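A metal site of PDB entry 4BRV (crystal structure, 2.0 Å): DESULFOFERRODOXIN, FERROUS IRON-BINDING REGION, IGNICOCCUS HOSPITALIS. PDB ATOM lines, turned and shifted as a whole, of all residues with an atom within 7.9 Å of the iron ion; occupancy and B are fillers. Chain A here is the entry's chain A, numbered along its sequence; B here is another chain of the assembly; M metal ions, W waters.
Of the 17 residues printed, 5 come within 4 Å of the iron ion.
The nearest printed residue that does not touch the iron ion is Lys 21 (4.5 Å).
The iron ion is bound by NE2 of His 56, 2.2 Å away.
The iron ion is bound by NE2 of His 25 (2.2 Å).
A ring nitrogen (NE2) of His 50 is bound to the iron ion.
Water W1 is bound to the iron ion (2.2 Å).
The iron ion is bound by ND1 of His 112 (2.3 Å).
The iron ion is bound by SG of Cys 109, 2.6 Å away.
The backbone NH (N) of Leu 111 lies close to the side-chain sulfur (SG) of Cys 109, 3.6 Å away.
A ring nitrogen (ND1) of His 25 is in hydrogen-bond range of the backbone carbonyl oxygen (O) of Lys 21, 2.7 Å away.
The backbone carbonyl oxygen (O) of His 112 lies within hydrogen-bond range of the indole nitrogen (NE1) of Trp 115.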
ATOM      1  N   LYS A  21       8.661   3.945  24.162  1.00  0.00           N
ATOM      2  CA  LYS A  21       9.083   4.863  23.103  1.00  0.00           C
ATOM      3  C   LYS A  21      10.577   5.232  23.205  1.00  0.00           C
ATOM      4  O   LYS A  21      11.128   5.867  22.303  1.00  0.00           O
ATOM      5  CB  LYS A  21       8.244   6.154  23.136  1.00  0.00           C
ATOM      6  CG  LYS A  21       6.739   5.960  23.051  1.00  0.00           C
ATOM      7  CD  LYS A  21       6.313   5.265  21.759  1.00  0.00           C
ATOM      8  CE  LYS A  21       6.401   6.198  20.555  1.00  0.00           C
ATOM      9  NZ  LYS A  21       6.392   5.493  19.236  1.00  0.00           N
ATOM     10  N   THR A  24      13.613   4.337  20.565  1.00  0.00           N
ATOM     11  CA  THR A  24      13.555   4.975  19.258  1.00  0.00           C
ATOM     12  C   THR A  24      13.476   6.522  19.286  1.00  0.00           C
ATOM     13  O   THR A  24      13.386   7.154  18.234  1.00  0.00           O
ATOM     14  CB  THR A  24      12.369   4.457  18.442  1.00  0.00           C
ATOM     15  OG1 THR A  24      11.170   4.609  19.222  1.00  0.00           O
ATOM     16  CG2 THR A  24      12.576   2.968  18.092  1.00  0.00           C
ATOM     17  N   HIS A  25      13.483   7.116  20.473  1.00  0.00           N
ATOM     18  CA  HIS A  25      13.509   8.568  20.559  1.00  0.00           C
ATOM     19  C   HIS A  25      14.767   9.140  21.231  1.00  0.00           C
ATOM     20  O   HIS A  25      15.147  10.262  20.934  1.00  0.00           O
ATOM     21  CB  HIS A  25      12.248   9.118  21.257  1.00  0.00           C
ATOM     22  CG  HIS A  25      10.989   8.916  20.466  1.00  0.00           C
ATOM     23  ND1 HIS A  25      10.272   7.746  20.503  1.00  0.00           N
ATOM     24  CD2 HIS A  25      10.323   9.742  19.621  1.00  0.00           C
ATOM     25  CE1 HIS A  25       9.206   7.859  19.729  1.00  0.00           C
ATOM     26  NE2 HIS A  25       9.217   9.062  19.181  1.00  0.00           N
ATOM     27  N   PRO A  49      15.571   3.720  14.907  1.00  0.00           N
ATOM     28  CA  PRO A  49      14.762   4.015  13.712  1.00  0.00           C
ATOM     29  C   PRO A  49      13.409   4.610  14.072  1.00  0.00           C
ATOM     30  O   PRO A  49      12.832   4.211  15.089  1.00  0.00           O
ATOM     31  CB  PRO A  49      14.569   2.632  13.052  1.00  0.00           C
ATOM     32  CG  PRO A  49      14.841   1.634  14.124  1.00  0.00           C
ATOM     33  CD  PRO A  49      15.875   2.287  15.013  1.00  0.00           C
ATOM     34  N   HIS A  50      12.933   5.546  13.258  1.00  0.00           N
ATOM     35  CA  HIS A  50      11.742   6.336  13.573  1.00  0.00           C
ATOM     36  C   HIS A  50      11.117   6.758  12.242  1.00  0.00           C
ATOM     37  O   HIS A  50      11.842   6.934  11.257  1.00  0.00           O
ATOM     38  CB  HIS A  50      12.179   7.553  14.385  1.00  0.00           C
ATOM     39  CG  HIS A  50      11.055   8.375  14.947  1.00  0.00           C
ATOM     40  ND1 HIS A  50      10.354   9.275  14.172  1.00  0.00           N
ATOM     41  CD2 HIS A  50      10.543   8.459  16.200  1.00  0.00           C
ATOM     42  CE1 HIS A  50       9.433   9.860  14.929  1.00  0.00           C
ATOM     43  NE2 HIS A  50       9.532   9.392  16.157  1.00  0.00           N
ATOM     44  N   PRO A  51       9.779   6.890  12.197  1.00  0.00           N
ATOM     45  CA  PRO A  51       9.202   7.430  10.963  1.00  0.00           C
ATOM     46  C   PRO A  51       9.704   8.862  10.642  1.00  0.00           C
ATOM     47  O   PRO A  51      10.212   9.571  11.524  1.00  0.00           O
ATOM     48  CB  PRO A  51       7.699   7.474  11.278  1.00  0.00           C
ATOM     49  CG  PRO A  51       7.505   6.435  12.364  1.00  0.00           C
ATOM     50  CD  PRO A  51       8.755   6.558  13.198  1.00  0.00           C
ATOM     51  N   HIS A  56       4.682  13.108  11.464  1.00  0.00           N
ATOM     52  CA  HIS A  56       5.411  12.451  12.557  1.00  0.00           C
ATOM     53  C   HIS A  56       6.888  12.323  12.205  1.00  0.00           C
ATOM     54  O   HIS A  56       7.264  11.481  11.366  1.00  0.00           O
ATOM     55  CB  HIS A  56       4.820  11.037  12.789  1.00  0.00           C
ATOM     56  CG  HIS A  56       5.428  10.323  13.967  1.00  0.00           C
ATOM     57  ND1 HIS A  56       5.198   8.985  14.222  1.00  0.00           N
ATOM     58  CD2 HIS A  56       6.242  10.772  14.957  1.00  0.00           C
ATOM     59  CE1 HIS A  56       5.856   8.634  15.326  1.00  0.00           C
ATOM     60  NE2 HIS A  56       6.490   9.697  15.779  1.00  0.00           N
ATOM     61  N   SER A  57       7.733  13.131  12.824  1.00  0.00           N
ATOM     62  CA  SER A  57       9.167  12.960  12.601  1.00  0.00           C
ATOM     63  C   SER A  57       9.982  13.569  13.733  1.00  0.00           C
ATOM     64  O   SER A  57       9.455  14.341  14.539  1.00  0.00           O
ATOM     65  CB  SER A  57       9.570  13.584  11.258  1.00  0.00           C
ATOM     66  OG  SER A  57       9.459  15.005  11.318  1.00  0.00           O
ATOM     67  N   ILE A  58      11.268  13.215  13.790  1.00  0.00           N
ATOM     68  CA  ILE A  58      12.204  13.930  14.650  1.00  0.00           C
ATOM     69  C   ILE A  58      12.456  15.274  13.956  1.00  0.00           C
ATOM     70  O   ILE A  58      13.082  15.308  12.892  1.00  0.00           O
ATOM     71  CB  ILE A  58      13.556  13.177  14.811  1.00  0.00           C
ATOM     72  CG1 ILE A  58      13.348  11.743  15.344  1.00  0.00           C
ATOM     73  CG2 ILE A  58      14.507  13.981  15.689  1.00  0.00           C
ATOM     74  CD1 ILE A  58      12.469  11.636  16.570  1.00  0.00           C
ATOM     75  N   TYR A 108      13.628  16.303  19.405  1.00  0.00           N
ATOM     76  CA  TYR A 108      12.194  16.567  19.546  1.00  0.00           C
ATOM     77  C   TYR A 108      11.414  15.830  18.485  1.00  0.00           C
ATOM     78  O   TYR A 108      11.698  15.939  17.277  1.00  0.00           O
ATOM     79  CB  TYR A 108      11.912  18.080  19.464  1.00  0.00           C
ATOM     80  CG  TYR A 108      10.439  18.458  19.431  1.00  0.00           C
ATOM     81  CD1 TYR A 108       9.698  18.513  20.607  1.00  0.00           C
ATOM     82  CD2 TYR A 108       9.790  18.792  18.235  1.00  0.00           C
ATOM     83  CE1 TYR A 108       8.325  18.870  20.597  1.00  0.00           C
ATOM     84  CE2 TYR A 108       8.425  19.165  18.210  1.00  0.00           C
ATOM     85  CZ  TYR A 108       7.706  19.196  19.400  1.00  0.00           C
ATOM     86  OH  TYR A 108       6.372  19.547  19.424  1.00  0.00           O
ATOM     87  N   CYS A 109      10.433  15.042  18.934  1.00  0.00           N
ATOM     88  CA  CYS A 109       9.467  14.415  18.052  1.00  0.00           C
ATOM     89  C   CYS A 109       8.145  15.182  18.204  1.00  0.00           C
ATOM     90  O   CYS A 109       7.692  15.402  19.334  1.00  0.00           O
ATOM     91  CB  CYS A 109       9.277  12.966  18.472  1.00  0.00           C
ATOM     92  SG  CYS A 109       7.922  12.083  17.620  1.00  0.00           S
ATOM     93  N   ASN A 110       7.512  15.570  17.096  1.00  0.00           N
ATOM     94  CA  ASN A 110       6.276  16.383  17.210  1.00  0.00           C
ATOM     95  C   ASN A 110       5.165  15.692  18.002  1.00  0.00           C
ATOM     96  O   ASN A 110       4.319  16.364  18.573  1.00  0.00           O
ATOM     97  CB  ASN A 110       5.740  16.843  15.827  1.00  0.00           C
ATOM     98  CG  ASN A 110       5.345  15.675  14.932  1.00  0.00           C
ATOM     99  OD1 ASN A 110       6.169  14.787  14.649  1.00  0.00           O
ATOM    100  ND2 ASN A 110       4.092  15.670  14.449  1.00  0.00           N
ATOM    101  N   LEU A 111       5.162  14.368  18.035  1.00  0.00           N
ATOM    102  CA  LEU A 111       4.133  13.612  18.775  1.00  0.00           C
ATOM    103  C   LEU A 111       4.595  13.203  20.172  1.00  0.00           C
ATOM    104  O   LEU A 111       3.766  13.072  21.089  1.00  0.00           O
ATOM    105  CB  LEU A 111       3.733  12.332  18.007  1.00  0.00           C
ATOM    106  CG  LEU A 111       2.977  12.467  16.697  1.00  0.00           C
ATOM    107  CD1 LEU A 111       2.562  11.083  16.167  1.00  0.00           C
ATOM    108  CD2 LEU A 111       1.749  13.388  16.856  1.00  0.00           C
ATOM    109  N   HIS A 112       5.888  12.958  20.328  1.00  0.00           N
ATOM    110  CA  HIS A 112       6.367  12.204  21.488  1.00  0.00           C
ATOM    111  C   HIS A 112       7.346  12.961  22.360  1.00  0.00           C
ATOM    112  O   HIS A 112       7.991  12.363  23.241  1.00  0.00           O
ATOM    113  CB  HIS A 112       6.927  10.854  21.013  1.00  0.00           C
ATOM    114  CG  HIS A 112       5.906  10.009  20.307  1.00  0.00           C
ATOM    115  ND1 HIS A 112       6.175   9.334  19.125  1.00  0.00           N
ATOM    116  CD2 HIS A 112       4.604   9.765  20.590  1.00  0.00           C
ATOM    117  CE1 HIS A 112       5.078   8.712  18.719  1.00  0.00           C
ATOM    118  NE2 HIS A 112       4.113   8.950  19.591  1.00  0.00           N
ATOM    119  N   GLY A 113       7.483  14.266  22.125  1.00  0.00           N
ATOM    120  CA  GLY A 113       8.114  15.155  23.082  1.00  0.00           C
ATOM    121  C   GLY A 113       9.625  15.243  22.984  1.00  0.00           C
ATOM    122  O   GLY A 113      10.206  14.958  21.926  1.00  0.00           O
ATOM    123  N   TRP A 115      13.515  14.358  24.217  1.00  0.00           N
ATOM    124  CA  TRP A 115      14.288  13.259  24.787  1.00  0.00           C
ATOM    125  C   TRP A 115      15.750  13.639  24.945  1.00  0.00           C
ATOM    126  O   TRP A 115      16.333  14.311  24.083  1.00  0.00           O
ATOM    127  CB  TRP A 115      14.153  12.022  23.900  1.00  0.00           C
ATOM    128  CG  TRP A 115      12.776  11.454  23.967  1.00  0.00           C
ATOM    129  CD1 TRP A 115      11.657  11.920  23.332  1.00  0.00           C
ATOM    130  CD2 TRP A 115      12.358  10.326  24.756  1.00  0.00           C
ATOM    131  NE1 TRP A 115      10.561  11.137  23.675  1.00  0.00           N
ATOM    132  CE2 TRP A 115      10.970  10.160  24.541  1.00  0.00           C
ATOM    133  CE3 TRP A 115      13.015   9.448  25.611  1.00  0.00           C
ATOM    134  CZ2 TRP A 115      10.245   9.147  25.163  1.00  0.00           C
ATOM    135  CZ3 TRP A 115      12.306   8.444  26.216  1.00  0.00           C
ATOM    136  CH2 TRP A 115      10.924   8.289  25.996  1.00  0.00           C
ATOM    137  N   PHE B  72       1.737  12.598  25.459  1.00  0.00           N
ATOM    138  CA  PHE B  72       3.115  13.056  25.673  1.00  0.00           C
ATOM    139  C   PHE B  72       3.133  14.568  25.620  1.00  0.00           C
ATOM    140  O   PHE B  72       2.230  15.172  25.051  1.00  0.00           O
ATOM    141  CB  PHE B  72       4.057  12.514  24.599  1.00  0.00           C
ATOM    142  CG  PHE B  72       4.134  11.004  24.554  1.00  0.00           C
ATOM    143  CD1 PHE B  72       3.160  10.264  23.918  1.00  0.00           C
ATOM    144  CD2 PHE B  72       5.207  10.343  25.137  1.00  0.00           C
ATOM    145  CE1 PHE B  72       3.238   8.870  23.854  1.00  0.00           C
ATOM    146  CE2 PHE B  72       5.293   8.939  25.082  1.00  0.00           C
ATOM    147  CZ  PHE B  72       4.303   8.210  24.448  1.00  0.00           C
HETATM  148 FE    FE M   1       7.781   9.470  17.548  1.00  0.00          FE
HETATM  149  O   HOH W   1       7.428   7.268  17.329  1.00  0.00           O
